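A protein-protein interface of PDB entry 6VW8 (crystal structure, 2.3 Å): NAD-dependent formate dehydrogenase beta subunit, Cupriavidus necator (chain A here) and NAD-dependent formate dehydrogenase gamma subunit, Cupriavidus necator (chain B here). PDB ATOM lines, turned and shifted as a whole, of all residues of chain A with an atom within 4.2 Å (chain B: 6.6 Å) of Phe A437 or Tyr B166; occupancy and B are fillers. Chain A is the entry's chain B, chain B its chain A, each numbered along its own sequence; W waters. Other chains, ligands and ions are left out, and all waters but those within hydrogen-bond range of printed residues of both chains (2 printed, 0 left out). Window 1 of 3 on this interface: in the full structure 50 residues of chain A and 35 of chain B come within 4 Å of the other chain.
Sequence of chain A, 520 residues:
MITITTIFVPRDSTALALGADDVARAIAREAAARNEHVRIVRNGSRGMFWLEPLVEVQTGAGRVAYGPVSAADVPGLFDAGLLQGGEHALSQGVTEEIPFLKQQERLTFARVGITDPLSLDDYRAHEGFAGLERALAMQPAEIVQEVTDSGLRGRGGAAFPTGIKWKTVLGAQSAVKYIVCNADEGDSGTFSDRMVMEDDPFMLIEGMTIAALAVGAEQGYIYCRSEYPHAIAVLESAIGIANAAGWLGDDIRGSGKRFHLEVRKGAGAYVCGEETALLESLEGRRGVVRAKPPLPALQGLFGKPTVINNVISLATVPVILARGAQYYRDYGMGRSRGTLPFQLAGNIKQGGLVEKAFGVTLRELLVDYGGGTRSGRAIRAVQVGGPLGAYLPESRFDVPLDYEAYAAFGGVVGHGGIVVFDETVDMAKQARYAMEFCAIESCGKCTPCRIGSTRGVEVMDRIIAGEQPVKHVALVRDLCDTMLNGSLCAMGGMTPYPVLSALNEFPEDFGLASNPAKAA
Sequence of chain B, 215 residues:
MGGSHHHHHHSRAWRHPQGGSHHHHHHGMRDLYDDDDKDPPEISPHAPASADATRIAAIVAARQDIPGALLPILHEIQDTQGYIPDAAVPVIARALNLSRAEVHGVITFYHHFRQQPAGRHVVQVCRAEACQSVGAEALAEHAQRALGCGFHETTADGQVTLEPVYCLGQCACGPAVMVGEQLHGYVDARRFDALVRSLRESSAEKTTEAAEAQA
The side-chain carboxylate (OE2) of Glu A436 lies within salt-bridge range of the guanidinium group (NH2) of Arg B127 (3.0 Å).
NH2 of Arg A225 sits at hydrogen-bond distance from O of Tyr B166, 3.1 Å away.
O of Cys B167 sits at hydrogen-bond distance from NH1 of Arg A225, 2.6 Å away.
The backbone NH of Ala B128 lies close to the side-chain sulfur of Cys B126, 3.4 Å away.
N of Cys B167 sits close to SG of Cys B126.
The backbone NH (N) of Arg B127 lies within hydrogen-bond range of the backbone carbonyl oxygen (O) of Val B165 (2.9 Å).
SG of Cys B167 sits close to N of Gly B169 (3.4 Å).
N of Tyr A270 sits at hydrogen-bond distance from OE1 of Glu A441, at 2.9 Å.
Pro A387 touches Glu B129.
Tyr A433 touches Arg B127.
Tyr A433 touches Ala B128.
Tyr A433 touches Glu B129.
Tyr A433 touches Tyr B166 (OH to CD1, 3.4 Å).
CE1 of Phe A437 touches CB of Tyr B166 (3.9 Å).
OH of Tyr B166 touches CD1 of Ile A440, at 3.3 Å.
Glu A441 touches Tyr B166 (OE2 to CD2, 3.7 Å).
Phe A437 touches one residue of chain B.
Printed residues of chain B within 4 Å of Glu A436: Arg B127 (3.0 Å).
Of the printed residues of chain B, Pro A387 touches Glu B129.
Val B125 touches none of the printed residues of chain A.
Val B165 touches none of the printed residues of chain A.
The nearest residue of chain A that does not touch Tyr B166 is Gly A186 (4.1 Å).
The nearest printed residue of chain B that does not touch Glu A436 is Tyr B166 (5.0 Å).
Among the printed residues, 11 pairs touch across the chains.
Among the printed residues, Asp or Glu carboxylates within 4 Å of a Lys or Arg side-chain nitrogen of the other chain: Glu A436 with Arg B127 (3.0 Å).
Water W2 lies within hydrogen-bond range of OH of Tyr A433 and OE1 of Glu B129.
Water W1 lies within hydrogen-bond range of the backbone carbonyl oxygen of Tyr B166 (2.6 Å), the backbone carbonyl oxygen of Gly A186 (2.6 Å) and the guanidinium group of Arg A225 (3.2 Å).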
ATOM      1  N   GLY A 186       0.267  17.472   1.590  1.00  0.00           N
ATOM      2  CA  GLY A 186       0.713  16.328   2.361  1.00  0.00           C
ATOM      3  C   GLY A 186       2.033  16.508   3.061  1.00  0.00           C
ATOM      4  O   GLY A 186       2.355  15.711   3.951  1.00  0.00           O
ATOM      5  N   ARG A 225      -7.121  17.265   2.177  1.00  0.00           N
ATOM      6  CA  ARG A 225      -6.707  16.108   2.971  1.00  0.00           C
ATOM      7  C   ARG A 225      -7.641  15.931   4.171  1.00  0.00           C
ATOM      8  O   ARG A 225      -8.236  16.893   4.674  1.00  0.00           O
ATOM      9  CB  ARG A 225      -5.253  16.275   3.435  1.00  0.00           C
ATOM     10  CG  ARG A 225      -4.984  17.530   4.285  1.00  0.00           C
ATOM     11  CD  ARG A 225      -3.465  17.885   4.446  1.00  0.00           C
ATOM     12  NE  ARG A 225      -2.612  16.699   4.609  1.00  0.00           N
ATOM     13  CZ  ARG A 225      -1.860  16.448   5.677  1.00  0.00           C
ATOM     14  NH1 ARG A 225      -1.829  17.311   6.692  1.00  0.00           N
ATOM     15  NH2 ARG A 225      -1.120  15.341   5.728  1.00  0.00           N
ATOM     16  N   TYR A 270      -0.858  10.087   1.538  1.00  0.00           N
ATOM     17  CA  TYR A 270       0.033  11.132   1.024  1.00  0.00           C
ATOM     18  C   TYR A 270       0.108  11.109  -0.506  1.00  0.00           C
ATOM     19  O   TYR A 270       0.088  12.167  -1.153  1.00  0.00           O
ATOM     20  CB  TYR A 270       1.432  10.975   1.653  1.00  0.00           C
ATOM     21  CG  TYR A 270       2.504  11.906   1.104  1.00  0.00           C
ATOM     22  CD1 TYR A 270       2.460  13.267   1.360  1.00  0.00           C
ATOM     23  CD2 TYR A 270       3.544  11.416   0.318  1.00  0.00           C
ATOM     24  CE1 TYR A 270       3.419  14.124   0.865  1.00  0.00           C
ATOM     25  CE2 TYR A 270       4.535  12.265  -0.186  1.00  0.00           C
ATOM     26  CZ  TYR A 270       4.460  13.623   0.096  1.00  0.00           C
ATOM     27  OH  TYR A 270       5.391  14.495  -0.408  1.00  0.00           O
ATOM     28  N   PRO A 387       8.962  16.147   2.802  1.00  0.00           N
ATOM     29  CA  PRO A 387       9.659  14.870   3.034  1.00  0.00           C
ATOM     30  C   PRO A 387      10.434  14.371   1.837  1.00  0.00           C
ATOM     31  O   PRO A 387      11.352  13.559   2.022  1.00  0.00           O
ATOM     32  CB  PRO A 387       8.527  13.905   3.417  1.00  0.00           C
ATOM     33  CG  PRO A 387       7.274  14.600   3.024  1.00  0.00           C
ATOM     34  CD  PRO A 387       7.537  16.059   3.122  1.00  0.00           C
ATOM     35  N   TYR A 433      13.586   7.062   8.533  1.00  0.00           N
ATOM     36  CA  TYR A 433      12.214   7.538   8.452  1.00  0.00           C
ATOM     37  C   TYR A 433      11.810   7.814   7.014  1.00  0.00           C
ATOM     38  O   TYR A 433      10.655   7.578   6.636  1.00  0.00           O
ATOM     39  CB  TYR A 433      12.019   8.793   9.296  1.00  0.00           C
ATOM     40  CG  TYR A 433      10.636   9.368   9.075  1.00  0.00           C
ATOM     41  CD1 TYR A 433       9.532   8.869   9.775  1.00  0.00           C
ATOM     42  CD2 TYR A 433      10.420  10.376   8.136  1.00  0.00           C
ATOM     43  CE1 TYR A 433       8.265   9.385   9.571  1.00  0.00           C
ATOM     44  CE2 TYR A 433       9.157  10.887   7.916  1.00  0.00           C
ATOM     45  CZ  TYR A 433       8.087  10.397   8.634  1.00  0.00           C
ATOM     46  OH  TYR A 433       6.839  10.923   8.411  1.00  0.00           O
ATOM     47  N   ALA A 434      12.723   8.379   6.215  1.00  0.00           N
ATOM     48  CA  ALA A 434      12.406   8.616   4.811  1.00  0.00           C
ATOM     49  C   ALA A 434      12.027   7.313   4.122  1.00  0.00           C
ATOM     50  O   ALA A 434      11.055   7.258   3.364  1.00  0.00           O
ATOM     51  CB  ALA A 434      13.585   9.285   4.091  1.00  0.00           C
ATOM     52  N   MET A 435      12.813   6.256   4.349  1.00  0.00           N
ATOM     53  CA  MET A 435      12.459   4.949   3.808  1.00  0.00           C
ATOM     54  C   MET A 435      11.148   4.441   4.410  1.00  0.00           C
ATOM     55  O   MET A 435      10.289   3.914   3.692  1.00  0.00           O
ATOM     56  CB  MET A 435      13.596   3.956   4.053  1.00  0.00           C
ATOM     57  CG  MET A 435      14.839   4.205   3.223  1.00  0.00           C
ATOM     58  SD  MET A 435      14.641   3.878   1.452  1.00  0.00           S
ATOM     59  CE  MET A 435      16.268   4.283   0.815  1.00  0.00           C
ATOM     60  N   GLU A 436      10.969   4.606   5.723  1.00  0.00           N
ATOM     61  CA  GLU A 436       9.745   4.143   6.378  1.00  0.00           C
ATOM     62  C   GLU A 436       8.523   4.869   5.833  1.00  0.00           C
ATOM     63  O   GLU A 436       7.524   4.238   5.460  1.00  0.00           O
ATOM     64  CB  GLU A 436       9.857   4.345   7.888  1.00  0.00           C
ATOM     65  CG  GLU A 436       8.845   3.563   8.695  1.00  0.00           C
ATOM     66  CD  GLU A 436       8.524   4.214  10.031  1.00  0.00           C
ATOM     67  OE1 GLU A 436       9.359   5.001  10.532  1.00  0.00           O
ATOM     68  OE2 GLU A 436       7.439   3.930  10.581  1.00  0.00           O
ATOM     69  N   PHE A 437       8.602   6.203   5.756  1.00  0.00           N
ATOM     70  CA  PHE A 437       7.515   6.999   5.186  1.00  0.00           C
ATOM     71  C   PHE A 437       7.171   6.534   3.775  1.00  0.00           C
ATOM     72  O   PHE A 437       6.003   6.582   3.368  1.00  0.00           O
ATOM     73  CB  PHE A 437       7.895   8.481   5.168  1.00  0.00           C
ATOM     74  CG  PHE A 437       6.782   9.386   4.735  1.00  0.00           C
ATOM     75  CD1 PHE A 437       5.570   9.426   5.462  1.00  0.00           C
ATOM     76  CD2 PHE A 437       6.920  10.198   3.611  1.00  0.00           C
ATOM     77  CE1 PHE A 437       4.515  10.267   5.072  1.00  0.00           C
ATOM     78  CE2 PHE A 437       5.871  11.043   3.209  1.00  0.00           C
ATOM     79  CZ  PHE A 437       4.648  11.073   3.962  1.00  0.00           C
ATOM     80  N   CYS A 438       8.176   6.128   2.990  1.00  0.00           N
ATOM     81  CA  CYS A 438       7.868   5.657   1.639  1.00  0.00           C
ATOM     82  C   CYS A 438       7.091   4.345   1.681  1.00  0.00           C
ATOM     83  O   CYS A 438       6.101   4.177   0.958  1.00  0.00           O
ATOM     84  CB  CYS A 438       9.149   5.489   0.811  1.00  0.00           C
ATOM     85  SG  CYS A 438       8.835   5.222  -0.985  1.00  0.00           S
ATOM     86  N   ALA A 439       7.501   3.421   2.553  1.00  0.00           N
ATOM     87  CA  ALA A 439       6.803   2.147   2.664  1.00  0.00           C
ATOM     88  C   ALA A 439       5.358   2.352   3.100  1.00  0.00           C
ATOM     89  O   ALA A 439       4.458   1.643   2.642  1.00  0.00           O
ATOM     90  CB  ALA A 439       7.539   1.229   3.635  1.00  0.00           C
ATOM     91  N   ILE A 440       5.120   3.329   3.977  1.00  0.00           N
ATOM     92  CA  ILE A 440       3.765   3.602   4.451  1.00  0.00           C
ATOM     93  C   ILE A 440       2.895   4.128   3.324  1.00  0.00           C
ATOM     94  O   ILE A 440       1.747   3.705   3.164  1.00  0.00           O
ATOM     95  CB  ILE A 440       3.792   4.579   5.643  1.00  0.00           C
ATOM     96  CG1 ILE A 440       4.396   3.889   6.868  1.00  0.00           C
ATOM     97  CG2 ILE A 440       2.340   5.097   5.975  1.00  0.00           C
ATOM     98  CD1 ILE A 440       4.951   4.832   7.934  1.00  0.00           C
ATOM     99  N   GLU A 441       3.402   5.078   2.539  1.00  0.00           N
ATOM    100  CA  GLU A 441       2.530   5.793   1.606  1.00  0.00           C
ATOM    101  C   GLU A 441       2.533   5.249   0.182  1.00  0.00           C
ATOM    102  O   GLU A 441       1.698   5.692  -0.612  1.00  0.00           O
ATOM    103  CB  GLU A 441       2.921   7.267   1.561  1.00  0.00           C
ATOM    104  CG  GLU A 441       3.014   7.888   2.908  1.00  0.00           C
ATOM    105  CD  GLU A 441       1.638   8.058   3.535  1.00  0.00           C
ATOM    106  OE1 GLU A 441       0.610   7.936   2.817  1.00  0.00           O
ATOM    107  OE2 GLU A 441       1.596   8.307   4.752  1.00  0.00           O
ATOM    108  N   HIS B 111      -5.948   4.908   4.747  1.00  0.00           N
ATOM    109  CA  HIS B 111      -5.729   4.734   6.181  1.00  0.00           C
ATOM    110  C   HIS B 111      -6.816   5.399   7.004  1.00  0.00           C
ATOM    111  O   HIS B 111      -7.083   4.962   8.127  1.00  0.00           O
ATOM    112  CB  HIS B 111      -4.375   5.284   6.636  1.00  0.00           C
ATOM    113  CG  HIS B 111      -4.164   5.141   8.115  1.00  0.00           C
ATOM    114  ND1 HIS B 111      -4.043   6.223   8.965  1.00  0.00           N
ATOM    115  CD2 HIS B 111      -4.126   4.038   8.907  1.00  0.00           C
ATOM    116  CE1 HIS B 111      -3.898   5.792  10.208  1.00  0.00           C
ATOM    117  NE2 HIS B 111      -3.944   4.471  10.200  1.00  0.00           N
ATOM    118  N   VAL B 125      -1.234  11.326  16.927  1.00  0.00           N
ATOM    119  CA  VAL B 125       0.065  11.903  17.268  1.00  0.00           C
ATOM    120  C   VAL B 125       0.853  12.073  15.969  1.00  0.00           C
ATOM    121  O   VAL B 125       1.213  11.082  15.313  1.00  0.00           O
ATOM    122  CB  VAL B 125       0.837  11.008  18.255  1.00  0.00           C
ATOM    123  CG1 VAL B 125       2.134  11.676  18.667  1.00  0.00           C
ATOM    124  CG2 VAL B 125      -0.018  10.682  19.483  1.00  0.00           C
ATOM    125  N   CYS B 126       1.141  13.316  15.603  1.00  0.00           N
ATOM    126  CA  CYS B 126       1.946  13.544  14.416  1.00  0.00           C
ATOM    127  C   CYS B 126       3.324  12.929  14.559  1.00  0.00           C
ATOM    128  O   CYS B 126       3.989  13.078  15.591  1.00  0.00           O
ATOM    129  CB  CYS B 126       2.102  15.017  14.123  1.00  0.00           C
ATOM    130  SG  CYS B 126       2.931  15.182  12.561  1.00  0.00           S
ATOM    131  N   ARG B 127       3.765  12.264  13.488  1.00  0.00           N
ATOM    132  CA  ARG B 127       5.078  11.624  13.435  1.00  0.00           C
ATOM    133  C   ARG B 127       5.974  12.171  12.332  1.00  0.00           C
ATOM    134  O   ARG B 127       7.046  11.600  12.097  1.00  0.00           O
ATOM    135  CB  ARG B 127       4.920  10.117  13.237  1.00  0.00           C
ATOM    136  CG  ARG B 127       4.547   9.373  14.505  1.00  0.00           C
ATOM    137  CD  ARG B 127       4.236   7.905  14.237  1.00  0.00           C
ATOM    138  NE  ARG B 127       5.134   7.309  13.254  1.00  0.00           N
ATOM    139  CZ  ARG B 127       6.224   6.620  13.569  1.00  0.00           C
ATOM    140  NH1 ARG B 127       6.541   6.447  14.853  1.00  0.00           N
ATOM    141  NH2 ARG B 127       6.995   6.115  12.606  1.00  0.00           N
ATOM    142  N   ALA B 128       5.583  13.247  11.639  1.00  0.00           N
ATOM    143  CA  ALA B 128       6.335  13.692  10.470  1.00  0.00           C
ATOM    144  C   ALA B 128       7.493  14.603  10.885  1.00  0.00           C
ATOM    145  O   ALA B 128       7.761  14.815  12.072  1.00  0.00           O
ATOM    146  CB  ALA B 128       5.419  14.368   9.454  1.00  0.00           C
ATOM    147  N   GLU B 129       8.187  15.168   9.896  1.00  0.00           N
ATOM    148  CA  GLU B 129       9.542  15.657  10.137  1.00  0.00           C
ATOM    149  C   GLU B 129       9.552  16.887  11.042  1.00  0.00           C
ATOM    150  O   GLU B 129      10.428  17.017  11.904  1.00  0.00           O
ATOM    151  CB  GLU B 129      10.235  15.947   8.800  1.00  0.00           C
ATOM    152  CG  GLU B 129      10.601  14.690   7.978  1.00  0.00           C
ATOM    153  CD  GLU B 129       9.436  14.161   7.122  1.00  0.00           C
ATOM    154  OE1 GLU B 129       8.255  14.438   7.434  1.00  0.00           O
ATOM    155  OE2 GLU B 129       9.690  13.440   6.139  1.00  0.00           O
ATOM    156  N   HIS B 152      -2.099   2.348  16.187  1.00  0.00           N
ATOM    157  CA  HIS B 152      -3.240   1.643  15.588  1.00  0.00           C
ATOM    158  C   HIS B 152      -3.909   0.693  16.579  1.00  0.00           C
ATOM    159  O   HIS B 152      -4.549  -0.280  16.180  1.00  0.00           O
ATOM    160  CB  HIS B 152      -2.862   0.869  14.314  1.00  0.00           C
ATOM    161  CG  HIS B 152      -1.788   1.514  13.486  1.00  0.00           C
ATOM    162  ND1 HIS B 152      -2.027   2.587  12.654  1.00  0.00           N
ATOM    163  CD2 HIS B 152      -0.474   1.216  13.345  1.00  0.00           C
ATOM    164  CE1 HIS B 152      -0.909   2.927  12.039  1.00  0.00           C
ATOM    165  NE2 HIS B 152       0.050   2.114  12.445  1.00  0.00           N
ATOM    166  N   PRO B 164      -1.082   7.181  14.463  1.00  0.00           N
ATOM    167  CA  PRO B 164      -0.142   8.141  13.894  1.00  0.00           C
ATOM    168  C   PRO B 164      -0.827   8.986  12.839  1.00  0.00           C
ATOM    169  O   PRO B 164      -1.792   8.567  12.205  1.00  0.00           O
ATOM    170  CB  PRO B 164       0.944   7.247  13.276  1.00  0.00           C
ATOM    171  CG  PRO B 164       0.186   6.016  12.829  1.00  0.00           C
ATOM    172  CD  PRO B 164      -1.070   5.900  13.728  1.00  0.00           C
ATOM    173  N   VAL B 165      -0.299  10.185  12.641  1.00  0.00           N
ATOM    174  CA  VAL B 165      -0.710  11.044  11.544  1.00  0.00           C
ATOM    175  C   VAL B 165       0.555  11.693  11.000  1.00  0.00           C
ATOM    176  O   VAL B 165       1.529  11.901  11.732  1.00  0.00           O
ATOM    177  CB  VAL B 165      -1.765  12.076  12.000  1.00  0.00           C
ATOM    178  CG1 VAL B 165      -1.218  12.904  13.142  1.00  0.00           C
ATOM    179  CG2 VAL B 165      -2.187  12.965  10.872  1.00  0.00           C
ATOM    180  N   TYR B 166       0.578  11.944   9.696  1.00  0.00           N
ATOM    181  CA  TYR B 166       1.771  12.490   9.064  1.00  0.00           C
ATOM    182  C   TYR B 166       1.477  13.936   8.685  1.00  0.00           C
ATOM    183  O   TYR B 166       1.119  14.249   7.541  1.00  0.00           O
ATOM    184  CB  TYR B 166       2.201  11.583   7.868  1.00  0.00           C
ATOM    185  CG  TYR B 166       2.450  10.199   8.419  1.00  0.00           C
ATOM    186  CD1 TYR B 166       3.624   9.927   9.093  1.00  0.00           C
ATOM    187  CD2 TYR B 166       1.464   9.200   8.386  1.00  0.00           C
ATOM    188  CE1 TYR B 166       3.858   8.690   9.673  1.00  0.00           C
ATOM    189  CE2 TYR B 166       1.693   7.946   8.959  1.00  0.00           C
ATOM    190  CZ  TYR B 166       2.900   7.704   9.604  1.00  0.00           C
ATOM    191  OH  TYR B 166       3.183   6.479  10.194  1.00  0.00           O
ATOM    192  N   CYS B 167       1.630  14.821   9.687  1.00  0.00           N
ATOM    193  CA  CYS B 167       1.463  16.271   9.565  1.00  0.00           C
ATOM    194  C   CYS B 167       0.002  16.709   9.661  1.00  0.00           C
ATOM    195  O   CYS B 167      -0.849  16.242   8.902  1.00  0.00           O
ATOM    196  CB  CYS B 167       2.086  16.780   8.258  1.00  0.00           C
ATOM    197  SG  CYS B 167       2.081  18.567   8.010  1.00  0.00           S
ATOM    198  N   LEU B 168      -0.295  17.573  10.638  1.00  0.00           N
ATOM    199  CA  LEU B 168      -1.593  18.223  10.825  1.00  0.00           C
ATOM    200  C   LEU B 168      -1.592  19.664  10.325  1.00  0.00           C
ATOM    201  O   LEU B 168      -2.555  20.394  10.575  1.00  0.00           O
ATOM    202  CB  LEU B 168      -1.969  18.196  12.304  1.00  0.00           C
ATOM    203  CG  LEU B 168      -2.099  16.774  12.837  1.00  0.00           C
ATOM    204  CD1 LEU B 168      -1.817  16.700  14.333  1.00  0.00           C
ATOM    205  CD2 LEU B 168      -3.487  16.235  12.509  1.00  0.00           C
ATOM    206  N   GLY B 169      -0.530  20.089   9.631  1.00  0.00           N
ATOM    207  CA  GLY B 169      -0.379  21.491   9.260  1.00  0.00           C
ATOM    208  C   GLY B 169      -0.137  22.387  10.461  1.00  0.00           C
ATOM    209  O   GLY B 169      -0.511  23.574  10.441  1.00  0.00           O
HETATM  210  O   HOH W   1       1.446  13.542   5.092  1.00  0.00           O
HETATM  211  O   HOH W   2       6.830  12.524   6.573  1.00  0.00           O
